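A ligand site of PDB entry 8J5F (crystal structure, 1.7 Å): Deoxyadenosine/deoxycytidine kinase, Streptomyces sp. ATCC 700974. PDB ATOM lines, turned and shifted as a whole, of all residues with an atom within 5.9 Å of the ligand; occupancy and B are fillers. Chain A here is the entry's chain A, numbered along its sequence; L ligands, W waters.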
ATOM      1  N   GLY A  35     -21.975 -23.392   7.317  1.00  0.00           N
ATOM      2  CA  GLY A  35     -20.727 -23.349   6.580  1.00  0.00           C
ATOM      3  C   GLY A  35     -20.043 -22.021   6.804  1.00  0.00           C
ATOM      4  O   GLY A  35     -20.619 -21.098   7.380  1.00  0.00           O
ATOM      5  N   ASN A  36     -18.795 -21.945   6.342  1.00  0.00           N
ATOM      6  CA  ASN A  36     -17.963 -20.777   6.598  1.00  0.00           C
ATOM      7  C   ASN A  36     -18.494 -19.535   5.862  1.00  0.00           C
ATOM      8  O   ASN A  36     -19.327 -19.605   4.946  1.00  0.00           O
ATOM      9  CB  ASN A  36     -16.516 -21.053   6.183  1.00  0.00           C
ATOM     10  CG  ASN A  36     -15.505 -20.222   6.981  1.00  0.00           C
ATOM     11  OD1 ASN A  36     -15.851 -19.595   7.979  1.00  0.00           O
ATOM     12  ND2 ASN A  36     -14.263 -20.216   6.517  1.00  0.00           N
ATOM     13  N   THR A  37     -17.978 -18.385   6.276  1.00  0.00           N
ATOM     14  CA  THR A  37     -18.401 -17.085   5.779  1.00  0.00           C
ATOM     15  C   THR A  37     -18.246 -16.980   4.254  1.00  0.00           C
ATOM     16  O   THR A  37     -17.346 -17.570   3.647  1.00  0.00           O
ATOM     17  CB  THR A  37     -17.572 -15.999   6.480  1.00  0.00           C
ATOM     18  OG1 THR A  37     -17.946 -14.695   6.028  1.00  0.00           O
ATOM     19  CG2 THR A  37     -16.055 -16.224   6.265  1.00  0.00           C
ATOM     20  N   ALA A  38     -19.176 -16.223   3.645  1.00  0.00           N
ATOM     21  CA  ALA A  38     -19.195 -15.939   2.201  1.00  0.00           C
ATOM     22  C   ALA A  38     -19.407 -17.207   1.365  1.00  0.00           C
ATOM     23  O   ALA A  38     -18.849 -17.380   0.282  1.00  0.00           O
ATOM     24  CB  ALA A  38     -17.942 -15.179   1.754  1.00  0.00           C
ATOM     25  N   ALA A  39     -20.276 -18.096   1.859  1.00  0.00           N
ATOM     26  CA  ALA A  39     -20.666 -19.286   1.133  1.00  0.00           C
ATOM     27  C   ALA A  39     -21.850 -19.054   0.201  1.00  0.00           C
ATOM     28  O   ALA A  39     -22.055 -19.835  -0.722  1.00  0.00           O
ATOM     29  CB  ALA A  39     -21.034 -20.410   2.117  1.00  0.00           C
ATOM     30  N   GLY A  40     -22.618 -17.999   0.435  1.00  0.00           N
ATOM     31  CA  GLY A  40     -23.874 -17.767  -0.237  1.00  0.00           C
ATOM     32  C   GLY A  40     -25.104 -18.029   0.625  1.00  0.00           C
ATOM     33  O   GLY A  40     -26.211 -18.177   0.066  1.00  0.00           O
ATOM     34  N   LYS A  41     -24.954 -18.087   1.947  1.00  0.00           N
ATOM     35  CA  LYS A  41     -26.072 -18.482   2.810  1.00  0.00           C
ATOM     36  C   LYS A  41     -27.164 -17.420   2.832  1.00  0.00           C
ATOM     37  O   LYS A  41     -28.355 -17.736   2.654  1.00  0.00           O
ATOM     38  CB  LYS A  41     -25.562 -18.778   4.228  1.00  0.00           C
ATOM     39  CG  LYS A  41     -24.382 -19.768   4.281  1.00  0.00           C
ATOM     40  CD  LYS A  41     -23.988 -20.203   5.695  1.00  0.00           C
ATOM     41  CE  LYS A  41     -23.136 -19.188   6.446  1.00  0.00           C
ATOM     42  NZ  LYS A  41     -21.932 -18.725   5.671  1.00  0.00           N
ATOM     43  N   THR A  42     -26.812 -16.144   3.056  1.00  0.00           N
ATOM     44  CA  THR A  42     -27.800 -15.064   3.090  1.00  0.00           C
ATOM     45  C   THR A  42     -28.666 -15.059   1.850  1.00  0.00           C
ATOM     46  O   THR A  42     -29.901 -14.983   1.919  1.00  0.00           O
ATOM     47  CB  THR A  42     -27.110 -13.701   3.214  1.00  0.00           C
ATOM     48  OG1 THR A  42     -26.269 -13.702   4.367  1.00  0.00           O
ATOM     49  CG2 THR A  42     -28.142 -12.592   3.348  1.00  0.00           C
ATOM     50  N   THR A  43     -28.012 -15.097   0.689  1.00  0.00           N
ATOM     51  CA  THR A  43     -28.705 -15.137  -0.595  1.00  0.00           C
ATOM     52  C   THR A  43     -29.757 -16.247  -0.615  1.00  0.00           C
ATOM     53  O   THR A  43     -30.906 -16.025  -1.013  1.00  0.00           O
ATOM     54  CB  THR A  43     -27.637 -15.344  -1.673  1.00  0.00           C
ATOM     55  OG1 THR A  43     -26.495 -14.520  -1.360  1.00  0.00           O
ATOM     56  CG2 THR A  43     -28.189 -15.007  -3.046  1.00  0.00           C
ATOM     57  N   LEU A  44     -29.371 -17.434  -0.159  1.00  0.00           N
ATOM     58  CA  LEU A  44     -30.263 -18.595  -0.188  1.00  0.00           C
ATOM     59  C   LEU A  44     -31.393 -18.448   0.832  1.00  0.00           C
ATOM     60  O   LEU A  44     -32.552 -18.773   0.551  1.00  0.00           O
ATOM     61  CB  LEU A  44     -29.420 -19.839   0.079  1.00  0.00           C
ATOM     62  CG  LEU A  44     -30.005 -21.245   0.223  1.00  0.00           C
ATOM     63  CD1 LEU A  44     -30.780 -21.618  -1.006  1.00  0.00           C
ATOM     64  CD2 LEU A  44     -28.865 -22.232   0.464  1.00  0.00           C
ATOM     65  N   GLU A 112     -29.246 -18.751   9.258  1.00  0.00           N
ATOM     66  CA  GLU A 112     -27.805 -18.787   9.041  1.00  0.00           C
ATOM     67  C   GLU A 112     -27.145 -19.481  10.227  1.00  0.00           C
ATOM     68  O   GLU A 112     -27.145 -18.936  11.341  1.00  0.00           O
ATOM     69  CB  GLU A 112     -27.264 -17.372   8.848  1.00  0.00           C
ATOM     70  CG  GLU A 112     -25.723 -17.340   8.800  1.00  0.00           C
ATOM     71  CD  GLU A 112     -25.156 -15.953   8.536  1.00  0.00           C
ATOM     72  OE1 GLU A 112     -25.918 -14.966   8.676  1.00  0.00           O
ATOM     73  OE2 GLU A 112     -23.958 -15.840   8.191  1.00  0.00           O
ATOM     74  N   MET A 159     -22.663 -26.583   3.627  1.00  0.00           N
ATOM     75  CA  MET A 159     -22.171 -25.774   2.501  1.00  0.00           C
ATOM     76  C   MET A 159     -20.907 -25.032   2.949  1.00  0.00           C
ATOM     77  O   MET A 159     -20.994 -23.856   3.319  1.00  0.00           O
ATOM     78  CB  MET A 159     -23.208 -24.752   2.044  1.00  0.00           C
ATOM     79  CG  MET A 159     -22.831 -24.101   0.730  1.00  0.00           C
ATOM     80  SD  MET A 159     -24.163 -23.228  -0.075  1.00  0.00           S
ATOM     81  CE  MET A 159     -24.579 -22.008   1.185  1.00  0.00           C
ATOM     82  N   ARG A 169     -14.891 -13.453  -2.522  1.00  0.00           N
ATOM     83  CA  ARG A 169     -16.191 -12.825  -2.375  1.00  0.00           C
ATOM     84  C   ARG A 169     -16.168 -11.700  -1.341  1.00  0.00           C
ATOM     85  O   ARG A 169     -16.792 -10.648  -1.541  1.00  0.00           O
ATOM     86  CB  ARG A 169     -17.221 -13.890  -1.993  1.00  0.00           C
ATOM     87  CG  ARG A 169     -17.461 -14.905  -3.099  1.00  0.00           C
ATOM     88  CD  ARG A 169     -18.366 -16.063  -2.636  1.00  0.00           C
ATOM     89  NE  ARG A 169     -18.662 -17.011  -3.706  1.00  0.00           N
ATOM     90  CZ  ARG A 169     -19.263 -18.182  -3.525  1.00  0.00           C
ATOM     91  NH1 ARG A 169     -19.630 -18.585  -2.315  1.00  0.00           N
ATOM     92  NH2 ARG A 169     -19.507 -18.967  -4.572  1.00  0.00           N
ATOM     93  N   LEU A 170     -15.449 -11.901  -0.233  1.00  0.00           N
ATOM     94  CA  LEU A 170     -15.388 -10.879   0.800  1.00  0.00           C
ATOM     95  C   LEU A 170     -14.661  -9.630   0.304  1.00  0.00           C
ATOM     96  O   LEU A 170     -15.072  -8.503   0.602  1.00  0.00           O
ATOM     97  CB  LEU A 170     -14.691 -11.396   2.054  1.00  0.00           C
ATOM     98  CG  LEU A 170     -15.453 -12.415   2.913  1.00  0.00           C
ATOM     99  CD1 LEU A 170     -14.511 -13.092   3.924  1.00  0.00           C
ATOM    100  CD2 LEU A 170     -16.641 -11.752   3.605  1.00  0.00           C
ATOM    101  N   ALA A 173     -16.937  -7.568  -1.971  1.00  0.00           N
ATOM    102  CA  ALA A 173     -17.995  -6.874  -1.248  1.00  0.00           C
ATOM    103  C   ALA A 173     -17.448  -5.715  -0.433  1.00  0.00           C
ATOM    104  O   ALA A 173     -18.031  -4.626  -0.414  1.00  0.00           O
ATOM    105  CB  ALA A 173     -18.759  -7.861  -0.347  1.00  0.00           C
ATOM    106  N   SER A 178     -20.425  -2.916  -0.073  1.00  0.00           N
ATOM    107  CA  SER A 178     -21.671  -3.627   0.204  1.00  0.00           C
ATOM    108  C   SER A 178     -21.597  -4.443   1.493  1.00  0.00           C
ATOM    109  O   SER A 178     -22.625  -4.985   1.926  1.00  0.00           O
ATOM    110  CB  SER A 178     -22.067  -4.539  -0.968  1.00  0.00           C
ATOM    111  OG  SER A 178     -21.044  -5.469  -1.287  1.00  0.00           O
ATOM    112  N   ARG A 179     -20.419  -4.551   2.113  1.00  0.00           N
ATOM    113  CA  ARG A 179     -20.332  -5.086   3.465  1.00  0.00           C
ATOM    114  C   ARG A 179     -19.227  -4.361   4.204  1.00  0.00           C
ATOM    115  O   ARG A 179     -18.241  -3.940   3.585  1.00  0.00           O
ATOM    116  CB  ARG A 179     -20.067  -6.601   3.492  1.00  0.00           C
ATOM    117  CG  ARG A 179     -18.623  -6.998   3.275  1.00  0.00           C
ATOM    118  CD  ARG A 179     -18.525  -8.503   3.208  1.00  0.00           C
ATOM    119  NE  ARG A 179     -18.559  -9.108   4.543  1.00  0.00           N
ATOM    120  CZ  ARG A 179     -19.431 -10.036   4.899  1.00  0.00           C
ATOM    121  NH1 ARG A 179     -20.383 -10.445   4.073  1.00  0.00           N
ATOM    122  NH2 ARG A 179     -19.358 -10.575   6.113  1.00  0.00           N
ATOM    123  N   ALA A 226     -20.469 -24.995  -2.262  1.00  0.00           N
ATOM    124  CA  ALA A 226     -20.522 -23.545  -2.120  1.00  0.00           C
ATOM    125  C   ALA A 226     -20.225 -22.818  -3.425  1.00  0.00           C
ATOM    126  O   ALA A 226     -20.556 -21.629  -3.540  1.00  0.00           O
ATOM    127  CB  ALA A 226     -19.532 -23.082  -1.049  1.00  0.00           C
ATOM    128  N   ALA A 227     -19.604 -23.486  -4.386  1.00  0.00           N
ATOM    129  CA  ALA A 227     -19.294 -22.905  -5.680  1.00  0.00           C
ATOM    130  C   ALA A 227     -20.434 -23.028  -6.684  1.00  0.00           C
ATOM    131  O   ALA A 227     -20.320 -22.514  -7.800  1.00  0.00           O
ATOM    132  CB  ALA A 227     -18.035 -23.557  -6.261  1.00  0.00           C
ATOM    133  N   ALA A 228     -21.526 -23.705  -6.318  1.00  0.00           N
ATOM    134  CA  ALA A 228     -22.659 -23.803  -7.222  1.00  0.00           C
ATOM    135  C   ALA A 228     -23.305 -22.436  -7.417  1.00  0.00           C
ATOM    136  O   ALA A 228     -23.185 -21.527  -6.590  1.00  0.00           O
ATOM    137  CB  ALA A 228     -23.692 -24.799  -6.695  1.00  0.00           C
ATOM    138  N   SER A 229     -24.021 -22.298  -8.539  1.00  0.00           N
ATOM    139  CA  SER A 229     -24.725 -21.052  -8.805  1.00  0.00           C
ATOM    140  C   SER A 229     -25.827 -20.860  -7.760  1.00  0.00           C
ATOM    141  O   SER A 229     -26.342 -21.830  -7.207  1.00  0.00           O
ATOM    142  CB  SER A 229     -25.340 -21.078 -10.208  1.00  0.00           C
ATOM    143  OG  SER A 229     -26.355 -22.071 -10.311  1.00  0.00           O
ATOM    144  N   PRO A 230     -26.189 -19.618  -7.465  1.00  0.00           N
ATOM    145  CA  PRO A 230     -27.290 -19.404  -6.516  1.00  0.00           C
ATOM    146  C   PRO A 230     -28.571 -20.102  -6.947  1.00  0.00           C
ATOM    147  O   PRO A 230     -29.313 -20.615  -6.106  1.00  0.00           O
ATOM    148  CB  PRO A 230     -27.456 -17.875  -6.481  1.00  0.00           C
ATOM    149  CG  PRO A 230     -26.366 -17.303  -7.305  1.00  0.00           C
ATOM    150  CD  PRO A 230     -25.428 -18.381  -7.731  1.00  0.00           C
ATOM    151  N   LYS A 233     -28.340 -23.704  -6.039  1.00  0.00           N
ATOM    152  CA  LYS A 233     -28.481 -23.892  -4.597  1.00  0.00           C
ATOM    153  C   LYS A 233     -29.944 -23.830  -4.172  1.00  0.00           C
ATOM    154  O   LYS A 233     -30.401 -24.657  -3.376  1.00  0.00           O
ATOM    155  CB  LYS A 233     -27.667 -22.832  -3.851  1.00  0.00           C
ATOM    156  CG  LYS A 233     -26.177 -22.996  -4.038  1.00  0.00           C
ATOM    157  CD  LYS A 233     -25.404 -22.064  -3.133  1.00  0.00           C
ATOM    158  CE  LYS A 233     -23.902 -22.104  -3.430  1.00  0.00           C
ATOM    159  NZ  LYS A 233     -23.215 -20.857  -2.977  1.00  0.00           N
HETATM  160  P1  LIG L   1     -22.756 -15.922   3.600  1.00  0.00           P
HETATM  161  O1  LIG L   1     -24.076 -15.604   4.185  1.00  0.00           O
HETATM  162  O2  LIG L   1     -22.530 -17.355   3.565  1.00  0.00           O
HETATM  163  O3  LIG L   1     -21.732 -15.357   4.498  1.00  0.00           O
HETATM  164  P2  LIG L   1     -23.518 -14.202   1.366  1.00  0.00           P
HETATM  165  O4  LIG L   1     -24.752 -14.752   0.817  1.00  0.00           O
HETATM  166  O5  LIG L   1     -23.915 -13.100   2.246  1.00  0.00           O
HETATM  167  O6  LIG L   1     -22.612 -15.361   2.082  1.00  0.00           O
HETATM  168  O7  LIG L   1     -22.481 -13.715   0.197  1.00  0.00           O
HETATM  169  C1  LIG L   1     -21.367 -12.955   0.567  1.00  0.00           C
HETATM  170  C2  LIG L   1     -20.869 -12.273  -0.659  1.00  0.00           C
HETATM  171  O8  LIG L   1     -20.572 -13.275  -1.662  1.00  0.00           O
HETATM  172  C3  LIG L   1     -21.938 -11.404  -1.245  1.00  0.00           C
HETATM  173  O9  LIG L   1     -21.326 -10.212  -1.762  1.00  0.00           O
HETATM  174  C4  LIG L   1     -22.532 -12.218  -2.339  1.00  0.00           C
HETATM  175  O10 LIG L   1     -23.098 -11.386  -3.348  1.00  0.00           O
HETATM  176  C5  LIG L   1     -21.393 -13.061  -2.847  1.00  0.00           C
HETATM  177  N1  LIG L   1     -21.823 -14.310  -3.377  1.00  0.00           N
HETATM  178  C6  LIG L   1     -22.676 -15.100  -2.744  1.00  0.00           C
HETATM  179  N2  LIG L   1     -22.918 -16.232  -3.434  1.00  0.00           N
HETATM  180  C7  LIG L   1     -22.078 -16.079  -4.637  1.00  0.00           C
HETATM  181  C8  LIG L   1     -21.841 -16.832  -5.752  1.00  0.00           C
HETATM  182  N3  LIG L   1     -22.493 -18.125  -5.932  1.00  0.00           N
HETATM  183  N4  LIG L   1     -21.000 -16.410  -6.670  1.00  0.00           N
HETATM  184  C9  LIG L   1     -20.417 -15.221  -6.478  1.00  0.00           C
HETATM  185  N5  LIG L   1     -20.553 -14.365  -5.433  1.00  0.00           N
HETATM  186  C10 LIG L   1     -21.401 -14.830  -4.532  1.00  0.00           C
HETATM  187  O   HOH W   1     -18.927 -10.491  -3.355  1.00  0.00           O
HETATM  188  O   HOH W   2     -24.144 -13.773   6.230  1.00  0.00           O
HETATM  189  O   HOH W   3     -20.598 -14.226   6.487  1.00  0.00           O
HETATM  190  O   HOH W   4     -20.594 -17.143  -9.466  1.00  0.00           O
HETATM  191  O   HOH W   5     -22.742 -12.244   4.841  1.00  0.00           O
HETATM  192  O   HOH W   6     -22.478  -9.472  -4.761  1.00  0.00           O
HETATM  193  O   HOH W   7     -24.274 -18.622  -3.678  1.00  0.00           O
HETATM  194  O   HOH W   8     -22.243  -7.847  -0.549  1.00  0.00           O
HETATM  195  O   HOH W   9     -24.776 -10.677   1.596  1.00  0.00           O
HETATM  196  O   HOH W  10     -17.209 -16.319  -6.274  1.00  0.00           O
HETATM  197  O   HOH W  11     -21.586 -16.653   7.347  1.00  0.00           O
HETATM  198  O   HOH W  12     -18.787 -12.227  -5.480  1.00  0.00           O
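O of Ala 38 sits at hydrogen-bond distance from NH1 of Arg 169, at 3.0 Å. NH1 of Arg 169 sits at hydrogen-bond distance from O of Ala 39 (3.2 Å). O of Ala 173 is in hydrogen-bond range of N of Arg 179 (3.5 Å). NZ of Lys 233 sits at hydrogen-bond distance from O of Ala 39 (2.7 Å). NZ of Lys 41 is in hydrogen-bond range of O of Asn 36, 2.8 Å away. NH2 of Arg 169 lies within hydrogen-bond range of O of Ala 226, at 3.0 Å. The backbone carbonyl oxygen of Ala 173 is in hydrogen-bond range of the backbone NH of Ser 178 (3.0 Å). NZ of Lys 41 lies within hydrogen-bond range of O of Gly 35 (3.2 Å).
Water W3 lies within hydrogen-bond range of an oxygen (O3) of the ligand (2.6 Å) and the side-chain hydroxyl of Thr 37 (2.7 Å). Water W2 lies within hydrogen-bond range of an oxygen (O1) of the ligand (2.7 Å), the side-chain hydroxyl (OG1) of Thr 42 (2.8 Å) and the side-chain carboxylate (OE2) of Glu 112 (2.9 Å). Water W7 bridges NZ of Lys 233 (2.6 Å) and N2 of the ligand (2.8 Å). Water W1 bridges O of Arg 169 (2.8 Å) and O9 of the ligand (2.9 Å). Water W5 lies within hydrogen-bond range of O5 of the ligand (3.0 Å) and NH1 of Arg 179 (3.1 Å). Water W11 lies within hydrogen-bond range of OE2 of Glu 112 (2.6 Å), NZ of Lys 41 (2.7 Å) and O3 of the ligand (3.1 Å).
NZ of Lys 41 is in salt-bridge range of O2 of the ligand (2.6 Å). The backbone NH (N) of Ala 38 lies within hydrogen-bond range of an oxygen (O3) of the ligand (2.8 Å). N of Lys 41 sits at hydrogen-bond distance from O2 of the ligand (3.0 Å). N of Thr 43 sits at hydrogen-bond distance from O4 of the ligand (3.3 Å). An oxygen (O4) of the ligand lies within hydrogen-bond range of the side-chain hydroxyl (OG1) of Thr 43 (2.8 Å). An oxygen (O2) of the ligand is in hydrogen-bond range of the backbone NH (N) of Ala 39 (2.9 Å). The backbone NH (N) of Thr 42 is in hydrogen-bond range of an oxygen (O1) of the ligand, 3.0 Å away. The side-chain hydroxyl (OG1) of Thr 42 sits at hydrogen-bond distance from an oxygen (O1) of the ligand (2.9 Å). N of Gly 40 sits at hydrogen-bond distance from O6 of the ligand, at 3.1 Å.
The guanidinium group (NH2) of Arg 169 sits close to a nitrogen (N3) of the ligand (3.4 Å). Residues that only touch the ligand: Thr 37, Ala 173, Ala 228 and Pro 230. Hydrophobic or aromatic side chains that line the ligand: Ala 39, Ala 173 and Pro 230. Within 4 Å of the ligand: Thr 37, Ala 38, Ala 39, Gly 40, Lys 41, Thr 42, Thr 43, Arg 169, Ala 173, Ala 228 and Pro 230. The nearest printed residue that does not touch the ligand is Glu 112 (4.01 Å).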
